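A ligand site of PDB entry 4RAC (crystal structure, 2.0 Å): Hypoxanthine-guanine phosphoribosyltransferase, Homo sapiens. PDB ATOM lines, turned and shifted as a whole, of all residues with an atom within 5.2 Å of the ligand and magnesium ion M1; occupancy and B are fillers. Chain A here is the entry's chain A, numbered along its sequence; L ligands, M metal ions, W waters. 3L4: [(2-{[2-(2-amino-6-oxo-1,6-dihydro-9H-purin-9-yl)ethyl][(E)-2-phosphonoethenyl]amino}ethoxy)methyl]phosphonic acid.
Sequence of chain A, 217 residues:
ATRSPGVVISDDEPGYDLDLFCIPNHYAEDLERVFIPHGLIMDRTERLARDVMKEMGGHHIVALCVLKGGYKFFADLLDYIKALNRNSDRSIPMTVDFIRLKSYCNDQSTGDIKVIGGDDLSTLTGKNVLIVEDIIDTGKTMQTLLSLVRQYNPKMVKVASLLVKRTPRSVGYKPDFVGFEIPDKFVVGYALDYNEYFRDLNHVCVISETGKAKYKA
N of Thr 141 is in hydrogen-bond range of OAE of the ligand, at 2.8 Å.
OAC of the ligand lies within hydrogen-bond range of OG1 of Thr 138.
An oxygen (OAF) of the ligand lies within hydrogen-bond range of the backbone NH (N) of Gly 139, at 2.7 Å.
N1 of the ligand sits at hydrogen-bond distance from O of Val 187 (2.7 Å).
The backbone carbonyl oxygen of Asp 193 lies within hydrogen-bond range of a nitrogen (N2) of the ligand (2.7 Å).
The backbone NH (N) of Lys 68 is in hydrogen-bond range of an oxygen (OAG) of the ligand (2.8 Å).
The backbone NH (N) of Gly 69 is in hydrogen-bond range of an oxygen (OAD) of the ligand (2.8 Å).
NZ of Lys 165 lies within hydrogen-bond range of O6 of the ligand (2.9 Å).
OAF of the ligand is in hydrogen-bond range of N of Asp 137 (2.9 Å).
The backbone NH (N) of Lys 140 is in hydrogen-bond range of an oxygen (OAE) of the ligand (3.5 Å).
An oxygen (OAG) of the ligand is in salt-bridge range of the guanidinium group (NH2) of Arg 199 (3.4 Å).
An oxygen (OAE) of the ligand is in hydrogen-bond range of the side-chain hydroxyl (OG1) of Thr 141 (2.5 Å).
The backbone NH of Thr 138 sits at hydrogen-bond distance from an oxygen (OAC) of the ligand, 2.9 Å away.
The backbone NH of Val 187 sits at hydrogen-bond distance from an oxygen (O6) of the ligand.
OD2 of Asp 193 is in hydrogen-bond range of N of Glu 196 (2.6 Å).
N of Lys 165 is in hydrogen-bond range of O of Ile 136 (3.0 Å).
The side-chain amino group of Lys 68 is in salt-bridge range of the side-chain carboxylate of Glu 196 (3.0 Å).
The backbone carbonyl oxygen (O) of Lys 185 lies within hydrogen-bond range of the side-chain amino group (NZ) of Lys 165 (3.2 Å).
NH2 of Arg 199 is in salt-bridge range of OD2 of Asp 193, at 3.3 Å.
The side-chain carboxylate (OE1) of Glu 196 lies within salt-bridge range of the guanidinium group (NE) of Arg 199 (3.1 Å).
OG1 of Thr 138 sits at hydrogen-bond distance from N of Lys 140 (3.2 Å).
The backbone carbonyl oxygen (O) of Lys 185 lies close to an oxygen (O6) of the ligand (3.4 Å).
C of Leu 67 touches OAG of the ligand, 3.7 Å away.
O of Leu 101 touches CAP of the ligand, 3.7 Å away.
Asp 134 touches the ligand.
Ile 135 touches the ligand (CD1 to O6, 3.7 Å).
Ile 136 touches the ligand.
CZ of Phe 186 touches C2 of the ligand, at 3.4 Å.
CB of Leu 192 touches N2 of the ligand, at 3.5 Å.
Hydrophobic or aromatic side chains within 4 Å of the ligand: Ile 135, Phe 186, Val 187 and Leu 192.
Within 4 Å of the ligand: Leu 67, Lys 68, Gly 69, Leu 101, Asp 134, Ile 135, Ile 136, Asp 137, Thr 138, Gly 139, Lys 140, Thr 141, Lys 165, Lys 185, Phe 186, Val 187, Leu 192, Asp 193 and Arg 199.
Of the 27 residues printed, 1 comes within 4 Å of magnesium ion M1.
Magnesium ion M1 is bound by water W5, 2.1 Å away.
Water W2 is bound to magnesium ion M1 (2.1 Å).
Water W3 is bound to magnesium ion M1, 2.1 Å away.
Magnesium ion M1 is bound by OAH of the ligand, at 2.2 Å.
Magnesium ion M1 is bound by water W9, at 2.3 Å.
The side-chain carboxylate (OD1) of Asp 193 is bound to magnesium ion M1 (2.3 Å).
Magnesium ion M1 has six donor atoms within binding distance.
Water W1 lies within hydrogen-bond range of OAF of the ligand (2.6 Å) and N of Met 142 (3.0 Å).
Water W12 lies within hydrogen-bond range of OAD of the ligand (2.7 Å), O of Val 66 (3.0 Å), N of Gly 69 (3.3 Å) and OD2 of Asp 134 (3.3 Å).
Water W8 lies within hydrogen-bond range of OAG of the ligand (2.7 Å), NE of Arg 100 (2.8 Å) and O of Leu 101 (3.1 Å).
Water W10 lies within hydrogen-bond range of an oxygen (OAG) of the ligand, the side-chain carboxylate of Glu 196, the guanidinium group of Arg 100 and the guanidinium group of Arg 199.
Water W4 lies within hydrogen-bond range of OD2 of Asp 134 (2.7 Å), OAD of the ligand (2.8 Å) and NH1 of Arg 199 (3.2 Å).
Water W6 bridges the side-chain carboxylate of Asp 134 (2.6 Å) and an oxygen (OAT) of the ligand (2.9 Å).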
ATOM      1  N   VAL A  66      20.573  -1.053 -27.190  1.00  0.00           N
ATOM      2  CA  VAL A  66      19.200  -1.498 -26.914  1.00  0.00           C
ATOM      3  C   VAL A  66      18.794  -1.177 -25.479  1.00  0.00           C
ATOM      4  O   VAL A  66      19.182  -1.872 -24.544  1.00  0.00           O
ATOM      5  CB  VAL A  66      18.975  -3.002 -27.213  1.00  0.00           C
ATOM      6  CG1 VAL A  66      17.498  -3.361 -27.036  1.00  0.00           C
ATOM      7  CG2 VAL A  66      19.420  -3.313 -28.629  1.00  0.00           C
ATOM      8  N   LEU A  67      18.046  -0.074 -25.340  1.00  0.00           N
ATOM      9  CA  LEU A  67      17.586   0.451 -24.060  1.00  0.00           C
ATOM     10  C   LEU A  67      16.510  -0.451 -23.462  1.00  0.00           C
ATOM     11  O   LEU A  67      15.797  -1.143 -24.199  1.00  0.00           O
ATOM     12  CB  LEU A  67      16.979   1.844 -24.295  1.00  0.00           C
ATOM     13  CG  LEU A  67      17.831   3.110 -24.156  1.00  0.00           C
ATOM     14  CD1 LEU A  67      19.306   2.852 -24.205  1.00  0.00           C
ATOM     15  CD2 LEU A  67      17.405   4.202 -25.197  1.00  0.00           C
ATOM     16  N   LYS A  68      16.361  -0.421 -22.135  1.00  0.00           N
ATOM     17  CA  LYS A  68      17.151   0.419 -21.243  1.00  0.00           C
ATOM     18  C   LYS A  68      18.388  -0.331 -20.747  1.00  0.00           C
ATOM     19  O   LYS A  68      19.443   0.254 -20.512  1.00  0.00           O
ATOM     20  CB  LYS A  68      16.313   0.821 -20.026  1.00  0.00           C
ATOM     21  CG  LYS A  68      15.074   1.707 -20.326  1.00  0.00           C
ATOM     22  CD  LYS A  68      14.421   2.067 -19.008  1.00  0.00           C
ATOM     23  CE  LYS A  68      13.110   2.809 -19.167  1.00  0.00           C
ATOM     24  NZ  LYS A  68      12.541   3.100 -17.810  1.00  0.00           N
ATOM     25  N   GLY A  69      18.226  -1.646 -20.595  1.00  0.00           N
ATOM     26  CA  GLY A  69      19.208  -2.454 -19.898  1.00  0.00           C
ATOM     27  C   GLY A  69      20.572  -2.505 -20.555  1.00  0.00           C
ATOM     28  O   GLY A  69      21.555  -2.865 -19.911  1.00  0.00           O
ATOM     29  N   GLY A  70      20.629  -2.144 -21.833  1.00  0.00           N
ATOM     30  CA  GLY A  70      21.873  -2.240 -22.565  1.00  0.00           C
ATOM     31  C   GLY A  70      22.809  -1.077 -22.318  1.00  0.00           C
ATOM     32  O   GLY A  70      23.976  -1.129 -22.710  1.00  0.00           O
ATOM     33  N   ARG A 100      14.688   1.148 -28.204  1.00  0.00           N
ATOM     34  CA  ARG A 100      14.098   0.468 -27.054  1.00  0.00           C
ATOM     35  C   ARG A 100      12.975  -0.500 -27.471  1.00  0.00           C
ATOM     36  O   ARG A 100      12.079  -0.142 -28.236  1.00  0.00           O
ATOM     37  CB  ARG A 100      13.579   1.491 -26.052  1.00  0.00           C
ATOM     38  CG  ARG A 100      12.880   0.866 -24.864  1.00  0.00           C
ATOM     39  CD  ARG A 100      12.509   1.924 -23.857  1.00  0.00           C
ATOM     40  NE  ARG A 100      11.768   1.321 -22.771  1.00  0.00           N
ATOM     41  CZ  ARG A 100      10.914   1.962 -21.988  1.00  0.00           C
ATOM     42  NH1 ARG A 100      10.700   3.265 -22.158  1.00  0.00           N
ATOM     43  NH2 ARG A 100      10.283   1.309 -21.038  1.00  0.00           N
ATOM     44  N   LEU A 101      13.046  -1.724 -26.957  1.00  0.00           N
ATOM     45  CA  LEU A 101      11.980  -2.705 -27.175  1.00  0.00           C
ATOM     46  C   LEU A 101      11.373  -3.049 -25.835  1.00  0.00           C
ATOM     47  O   LEU A 101      12.096  -3.326 -24.862  1.00  0.00           O
ATOM     48  CB  LEU A 101      12.532  -3.972 -27.827  1.00  0.00           C
ATOM     49  CG  LEU A 101      12.815  -3.901 -29.327  1.00  0.00           C
ATOM     50  CD1 LEU A 101      14.152  -3.232 -29.588  1.00  0.00           C
ATOM     51  CD2 LEU A 101      12.793  -5.294 -29.935  1.00  0.00           C
ATOM     52  N   LYS A 102      10.048  -3.045 -25.771  1.00  0.00           N
ATOM     53  CA  LYS A 102       9.359  -3.173 -24.494  1.00  0.00           C
ATOM     54  C   LYS A 102       8.310  -4.277 -24.481  1.00  0.00           C
ATOM     55  O   LYS A 102       7.518  -4.389 -25.402  1.00  0.00           O
ATOM     56  CB  LYS A 102       8.720  -1.831 -24.105  1.00  0.00           C
ATOM     57  CG  LYS A 102       8.098  -1.840 -22.732  1.00  0.00           C
ATOM     58  CD  LYS A 102       7.642  -0.443 -22.328  1.00  0.00           C
ATOM     59  CE  LYS A 102       6.993  -0.474 -20.951  1.00  0.00           C
ATOM     60  NZ  LYS A 102       7.851  -1.205 -19.960  1.00  0.00           N
ATOM     61  N   ASP A 134      21.870  -6.224 -23.260  1.00  0.00           N
ATOM     62  CA  ASP A 134      22.219  -6.689 -21.916  1.00  0.00           C
ATOM     63  C   ASP A 134      22.133  -8.226 -21.862  1.00  0.00           C
ATOM     64  O   ASP A 134      23.069  -8.884 -21.412  1.00  0.00           O
ATOM     65  CB  ASP A 134      21.307  -6.032 -20.849  1.00  0.00           C
ATOM     66  CG  ASP A 134      19.826  -6.123 -21.205  1.00  0.00           C
ATOM     67  OD1 ASP A 134      19.533  -6.498 -22.359  1.00  0.00           O
ATOM     68  OD2 ASP A 134      18.954  -5.836 -20.339  1.00  0.00           O
ATOM     69  N   ILE A 135      21.028  -8.785 -22.347  1.00  0.00           N
ATOM     70  CA  ILE A 135      20.769 -10.208 -22.154  1.00  0.00           C
ATOM     71  C   ILE A 135      19.947 -10.868 -23.266  1.00  0.00           C
ATOM     72  O   ILE A 135      19.096 -10.231 -23.876  1.00  0.00           O
ATOM     73  CB  ILE A 135      20.032 -10.424 -20.800  1.00  0.00           C
ATOM     74  CG1 ILE A 135      20.009 -11.888 -20.404  1.00  0.00           C
ATOM     75  CG2 ILE A 135      18.597  -9.833 -20.840  1.00  0.00           C
ATOM     76  CD1 ILE A 135      19.698 -12.069 -18.959  1.00  0.00           C
ATOM     77  N   ILE A 136      20.212 -12.151 -23.506  1.00  0.00           N
ATOM     78  CA  ILE A 136      19.365 -12.969 -24.348  1.00  0.00           C
ATOM     79  C   ILE A 136      18.764 -14.087 -23.518  1.00  0.00           C
ATOM     80  O   ILE A 136      19.491 -14.949 -23.002  1.00  0.00           O
ATOM     81  CB  ILE A 136      20.137 -13.586 -25.531  1.00  0.00           C
ATOM     82  CG1 ILE A 136      20.536 -12.485 -26.509  1.00  0.00           C
ATOM     83  CG2 ILE A 136      19.284 -14.662 -26.213  1.00  0.00           C
ATOM     84  CD1 ILE A 136      21.448 -12.960 -27.625  1.00  0.00           C
ATOM     85  N   ASP A 137      17.439 -14.064 -23.392  1.00  0.00           N
ATOM     86  CA  ASP A 137      16.678 -15.095 -22.695  1.00  0.00           C
ATOM     87  C   ASP A 137      15.963 -15.986 -23.715  1.00  0.00           C
ATOM     88  O   ASP A 137      16.528 -16.986 -24.174  1.00  0.00           O
ATOM     89  CB  ASP A 137      15.667 -14.453 -21.731  1.00  0.00           C
ATOM     90  CG  ASP A 137      14.991 -15.482 -20.806  1.00  0.00           C
ATOM     91  OD1 ASP A 137      15.528 -16.597 -20.646  1.00  0.00           O
ATOM     92  OD2 ASP A 137      13.930 -15.173 -20.228  1.00  0.00           O
ATOM     93  N   THR A 138      14.723 -15.640 -24.080  1.00  0.00           N
ATOM     94  CA  THR A 138      14.011 -16.461 -25.067  1.00  0.00           C
ATOM     95  C   THR A 138      14.566 -16.220 -26.458  1.00  0.00           C
ATOM     96  O   THR A 138      14.390 -17.028 -27.348  1.00  0.00           O
ATOM     97  CB  THR A 138      12.496 -16.179 -25.106  1.00  0.00           C
ATOM     98  OG1 THR A 138      12.266 -14.833 -25.531  1.00  0.00           O
ATOM     99  CG2 THR A 138      11.869 -16.378 -23.734  1.00  0.00           C
ATOM    100  N   GLY A 139      15.243 -15.084 -26.644  1.00  0.00           N
ATOM    101  CA  GLY A 139      15.729 -14.697 -27.956  1.00  0.00           C
ATOM    102  C   GLY A 139      14.691 -13.993 -28.830  1.00  0.00           C
ATOM    103  O   GLY A 139      15.007 -13.577 -29.937  1.00  0.00           O
ATOM    104  N   LYS A 140      13.472 -13.856 -28.323  1.00  0.00           N
ATOM    105  CA  LYS A 140      12.378 -13.287 -29.112  1.00  0.00           C
ATOM    106  C   LYS A 140      12.562 -11.791 -29.384  1.00  0.00           C
ATOM    107  O   LYS A 140      12.277 -11.314 -30.483  1.00  0.00           O
ATOM    108  CB  LYS A 140      11.035 -13.552 -28.458  1.00  0.00           C
ATOM    109  N   THR A 141      13.025 -11.053 -28.370  1.00  0.00           N
ATOM    110  CA  THR A 141      13.390  -9.657 -28.548  1.00  0.00           C
ATOM    111  C   THR A 141      14.430  -9.524 -29.650  1.00  0.00           C
ATOM    112  O   THR A 141      14.257  -8.748 -30.583  1.00  0.00           O
ATOM    113  CB  THR A 141      13.953  -9.070 -27.229  1.00  0.00           C
ATOM    114  OG1 THR A 141      13.014  -9.278 -26.172  1.00  0.00           O
ATOM    115  CG2 THR A 141      14.200  -7.588 -27.377  1.00  0.00           C
ATOM    116  N   MET A 142      15.510 -10.302 -29.555  1.00  0.00           N
ATOM    117  CA  MET A 142      16.569 -10.252 -30.572  1.00  0.00           C
ATOM    118  C   MET A 142      16.107 -10.587 -32.000  1.00  0.00           C
ATOM    119  O   MET A 142      16.464  -9.866 -32.935  1.00  0.00           O
ATOM    120  CB  MET A 142      17.758 -11.136 -30.202  1.00  0.00           C
ATOM    121  CG  MET A 142      18.938 -10.960 -31.143  1.00  0.00           C
ATOM    122  SD  MET A 142      19.427  -9.210 -31.268  1.00  0.00           S
ATOM    123  CE  MET A 142      20.041  -8.950 -29.628  1.00  0.00           C
ATOM    124  N   LYS A 165      21.455 -16.633 -21.449  1.00  0.00           N
ATOM    125  CA  LYS A 165      21.019 -17.649 -20.509  1.00  0.00           C
ATOM    126  C   LYS A 165      21.052 -19.025 -21.155  1.00  0.00           C
ATOM    127  O   LYS A 165      20.726 -19.164 -22.334  1.00  0.00           O
ATOM    128  CB  LYS A 165      19.598 -17.384 -20.018  1.00  0.00           C
ATOM    129  CG  LYS A 165      19.451 -16.276 -19.024  1.00  0.00           C
ATOM    130  CD  LYS A 165      18.088 -16.384 -18.356  1.00  0.00           C
ATOM    131  CE  LYS A 165      17.744 -15.068 -17.713  1.00  0.00           C
ATOM    132  NZ  LYS A 165      16.501 -15.123 -16.889  1.00  0.00           N
ATOM    133  N   LYS A 185      18.471 -18.166 -14.371  1.00  0.00           N
ATOM    134  CA  LYS A 185      18.102 -17.472 -13.140  1.00  0.00           C
ATOM    135  C   LYS A 185      17.845 -16.009 -13.486  1.00  0.00           C
ATOM    136  O   LYS A 185      18.463 -15.471 -14.395  1.00  0.00           O
ATOM    137  CB  LYS A 185      19.238 -17.543 -12.112  1.00  0.00           C
ATOM    138  CG  LYS A 185      19.447 -18.899 -11.441  1.00  0.00           C
ATOM    139  CD  LYS A 185      20.764 -18.896 -10.619  1.00  0.00           C
ATOM    140  CE  LYS A 185      20.946 -20.210  -9.812  1.00  0.00           C
ATOM    141  NZ  LYS A 185      22.322 -20.292  -9.180  1.00  0.00           N
ATOM    142  N   PHE A 186      16.943 -15.361 -12.754  1.00  0.00           N
ATOM    143  CA  PHE A 186      16.651 -13.961 -13.009  1.00  0.00           C
ATOM    144  C   PHE A 186      17.704 -13.071 -12.340  1.00  0.00           C
ATOM    145  O   PHE A 186      17.887 -13.122 -11.141  1.00  0.00           O
ATOM    146  CB  PHE A 186      15.229 -13.606 -12.550  1.00  0.00           C
ATOM    147  CG  PHE A 186      14.752 -12.270 -13.049  1.00  0.00           C
ATOM    148  CD1 PHE A 186      15.023 -11.100 -12.320  1.00  0.00           C
ATOM    149  CD2 PHE A 186      14.062 -12.157 -14.245  1.00  0.00           C
ATOM    150  CE1 PHE A 186      14.600  -9.861 -12.789  1.00  0.00           C
ATOM    151  CE2 PHE A 186      13.636 -10.921 -14.728  1.00  0.00           C
ATOM    152  CZ  PHE A 186      13.906  -9.764 -13.980  1.00  0.00           C
ATOM    153  N   VAL A 187      18.420 -12.274 -13.122  1.00  0.00           N
ATOM    154  CA  VAL A 187      19.484 -11.437 -12.553  1.00  0.00           C
ATOM    155  C   VAL A 187      19.146  -9.965 -12.752  1.00  0.00           C
ATOM    156  O   VAL A 187      18.341  -9.615 -13.615  1.00  0.00           O
ATOM    157  CB  VAL A 187      20.852 -11.749 -13.193  1.00  0.00           C
ATOM    158  CG1 VAL A 187      21.292 -13.170 -12.835  1.00  0.00           C
ATOM    159  CG2 VAL A 187      20.758 -11.581 -14.702  1.00  0.00           C
ATOM    160  N   VAL A 188      19.784  -9.119 -11.935  1.00  0.00           N
ATOM    161  CA  VAL A 188      19.569  -7.681 -11.933  1.00  0.00           C
ATOM    162  C   VAL A 188      20.902  -6.984 -11.694  1.00  0.00           C
ATOM    163  O   VAL A 188      21.899  -7.636 -11.318  1.00  0.00           O
ATOM    164  CB  VAL A 188      18.567  -7.219 -10.825  1.00  0.00           C
ATOM    165  CG1 VAL A 188      17.227  -7.888 -10.981  1.00  0.00           C
ATOM    166  CG2 VAL A 188      19.128  -7.479  -9.400  1.00  0.00           C
ATOM    167  N   LEU A 192      20.416  -3.972 -15.665  1.00  0.00           N
ATOM    168  CA  LEU A 192      19.258  -4.876 -15.765  1.00  0.00           C
ATOM    169  C   LEU A 192      18.332  -4.672 -14.575  1.00  0.00           C
ATOM    170  O   LEU A 192      18.799  -4.522 -13.456  1.00  0.00           O
ATOM    171  CB  LEU A 192      19.700  -6.335 -15.845  1.00  0.00           C
ATOM    172  CG  LEU A 192      20.379  -6.724 -17.160  1.00  0.00           C
ATOM    173  CD1 LEU A 192      21.879  -6.482 -17.079  1.00  0.00           C
ATOM    174  CD2 LEU A 192      20.064  -8.179 -17.506  1.00  0.00           C
ATOM    175  N   ASP A 193      17.030  -4.677 -14.818  1.00  0.00           N
ATOM    176  CA  ASP A 193      16.071  -4.278 -13.800  1.00  0.00           C
ATOM    177  C   ASP A 193      15.099  -5.358 -13.376  1.00  0.00           C
ATOM    178  O   ASP A 193      14.911  -6.358 -14.055  1.00  0.00           O
ATOM    179  CB  ASP A 193      15.235  -3.097 -14.305  1.00  0.00           C
ATOM    180  CG  ASP A 193      14.140  -3.535 -15.302  1.00  0.00           C
ATOM    181  OD1 ASP A 193      14.464  -4.221 -16.303  1.00  0.00           O
ATOM    182  OD2 ASP A 193      12.960  -3.188 -15.068  1.00  0.00           O
ATOM    183  N   TYR A 194      14.454  -5.101 -12.241  1.00  0.00           N
ATOM    184  CA  TYR A 194      13.224  -5.758 -11.863  1.00  0.00           C
ATOM    185  C   TYR A 194      12.222  -4.644 -11.638  1.00  0.00           C
ATOM    186  O   TYR A 194      12.337  -3.882 -10.664  1.00  0.00           O
ATOM    187  CB  TYR A 194      13.407  -6.575 -10.578  1.00  0.00           C
ATOM    188  CG  TYR A 194      12.137  -7.200 -10.051  1.00  0.00           C
ATOM    189  CD1 TYR A 194      11.451  -8.148 -10.793  1.00  0.00           C
ATOM    190  CD2 TYR A 194      11.650  -6.860  -8.791  1.00  0.00           C
ATOM    191  CE1 TYR A 194      10.287  -8.724 -10.308  1.00  0.00           C
ATOM    192  CE2 TYR A 194      10.499  -7.424  -8.297  1.00  0.00           C
ATOM    193  CZ  TYR A 194       9.814  -8.360  -9.058  1.00  0.00           C
ATOM    194  OH  TYR A 194       8.659  -8.926  -8.555  1.00  0.00           O
ATOM    195  N   GLU A 196      11.989  -1.795 -13.097  1.00  0.00           N
ATOM    196  CA  GLU A 196      12.722  -0.514 -13.117  1.00  0.00           C
ATOM    197  C   GLU A 196      13.714  -0.313 -11.961  1.00  0.00           C
ATOM    198  O   GLU A 196      14.552   0.604 -11.994  1.00  0.00           O
ATOM    199  CB  GLU A 196      11.790   0.692 -13.296  1.00  0.00           C
ATOM    200  CG  GLU A 196      10.984   0.653 -14.607  1.00  0.00           C
ATOM    201  CD  GLU A 196      11.878   0.473 -15.827  1.00  0.00           C
ATOM    202  OE1 GLU A 196      13.024   0.957 -15.829  1.00  0.00           O
ATOM    203  OE2 GLU A 196      11.427  -0.170 -16.788  1.00  0.00           O
ATOM    204  N   ARG A 199      18.624  -0.957 -11.539  1.00  0.00           N
ATOM    205  CA  ARG A 199      19.471  -0.501 -12.644  1.00  0.00           C
ATOM    206  C   ARG A 199      20.658   0.283 -12.093  1.00  0.00           C
ATOM    207  O   ARG A 199      21.748   0.253 -12.670  1.00  0.00           O
ATOM    208  CB  ARG A 199      18.692   0.322 -13.676  1.00  0.00           C
ATOM    209  CG  ARG A 199      17.623  -0.460 -14.468  1.00  0.00           C
ATOM    210  CD  ARG A 199      17.239   0.301 -15.742  1.00  0.00           C
ATOM    211  NE  ARG A 199      15.886  -0.023 -16.233  1.00  0.00           N
ATOM    212  CZ  ARG A 199      15.595  -1.068 -17.014  1.00  0.00           C
ATOM    213  NH1 ARG A 199      16.568  -1.903 -17.397  1.00  0.00           N
ATOM    214  NH2 ARG A 199      14.349  -1.291 -17.419  1.00  0.00           N
HETATM  215  OAG 3L4 L   1      14.278  -1.742 -20.826  1.00  0.00           O
HETATM  216  PBB 3L4 L   1      14.644  -3.220 -20.528  1.00  0.00           P
HETATM  217  OAH 3L4 L   1      14.390  -3.602 -19.047  1.00  0.00           O
HETATM  218  OAD 3L4 L   1      16.052  -3.445 -20.900  1.00  0.00           O
HETATM  219  CAP 3L4 L   1      13.486  -4.223 -21.578  1.00  0.00           C
HETATM  220  OAT 3L4 L   1      14.077  -5.284 -22.233  1.00  0.00           O
HETATM  221  CAJ 3L4 L   1      13.725  -6.528 -21.816  1.00  0.00           C
HETATM  222  CAK 3L4 L   1      13.740  -7.709 -22.786  1.00  0.00           C
HETATM  223  NAY 3L4 L   1      13.404  -8.839 -22.014  1.00  0.00           N
HETATM  224  CAM 3L4 L   1      13.413 -10.199 -22.689  1.00  0.00           C
HETATM  225  CAO 3L4 L   1      14.575 -10.778 -23.402  1.00  0.00           C
HETATM  226  PBA 3L4 L   1      14.100 -12.194 -24.435  1.00  0.00           P
HETATM  227  OAE 3L4 L   1      13.192 -11.724 -25.622  1.00  0.00           O
HETATM  228  OAF 3L4 L   1      15.321 -12.901 -25.080  1.00  0.00           O
HETATM  229  OAC 3L4 L   1      13.317 -13.161 -23.572  1.00  0.00           O
HETATM  230  CAL 3L4 L   1      14.253  -8.794 -20.750  1.00  0.00           C
HETATM  231  CAN 3L4 L   1      13.656  -9.570 -19.573  1.00  0.00           C
HETATM  232  N9  3L4 L   1      14.463 -10.569 -18.984  1.00  0.00           N
HETATM  233  C4  3L4 L   1      15.286 -10.310 -17.907  1.00  0.00           C
HETATM  234  N3  3L4 L   1      15.534  -9.149 -17.201  1.00  0.00           N
HETATM  235  C2  3L4 L   1      16.385  -9.151 -16.186  1.00  0.00           C
HETATM  236  N2  3L4 L   1      16.614  -7.914 -15.489  1.00  0.00           N
HETATM  237  N1  3L4 L   1      17.004 -10.294 -15.819  1.00  0.00           N
HETATM  238  C6  3L4 L   1      16.815 -11.463 -16.445  1.00  0.00           C
HETATM  239  O6  3L4 L   1      17.499 -12.594 -15.990  1.00  0.00           O
HETATM  240  C5  3L4 L   1      15.885 -11.472 -17.553  1.00  0.00           C
HETATM  241  N7  3L4 L   1      15.408 -12.439 -18.459  1.00  0.00           N
HETATM  242  C8  3L4 L   1      14.544 -11.873 -19.309  1.00  0.00           C
HETATM  243 MG    MG M   1      13.367  -5.205 -18.018  1.00  0.00          MG
HETATM  244 MG    MG M   2      17.707  -5.988 -23.343  1.00  0.00          MG
HETATM  245  O   HOH W   1      16.436 -11.820 -27.174  1.00  0.00           O
HETATM  246  O   HOH W   2      15.101  -6.271 -18.322  1.00  0.00           O
HETATM  247  O   HOH W   3      12.144  -6.302 -19.336  1.00  0.00           O
HETATM  248  O   HOH W   4      17.178  -4.736 -18.672  1.00  0.00           O
HETATM  249  O   HOH W   5      11.890  -3.934 -17.367  1.00  0.00           O
HETATM  250  O   HOH W   6      16.713  -6.307 -21.656  1.00  0.00           O
HETATM  251  O   HOH W   7      16.092  -5.821 -24.852  1.00  0.00           O
HETATM  252  O   HOH W   8      12.103  -1.405 -22.402  1.00  0.00           O
HETATM  253  O   HOH W   9      12.966  -6.670 -16.346  1.00  0.00           O
HETATM  254  O   HOH W  10      11.939  -0.795 -19.669  1.00  0.00           O
HETATM  255  O   HOH W  11      10.680 -11.614 -24.968  1.00  0.00           O
HETATM  256  O   HOH W  12      17.812  -3.961 -22.868  1.00  0.00           O
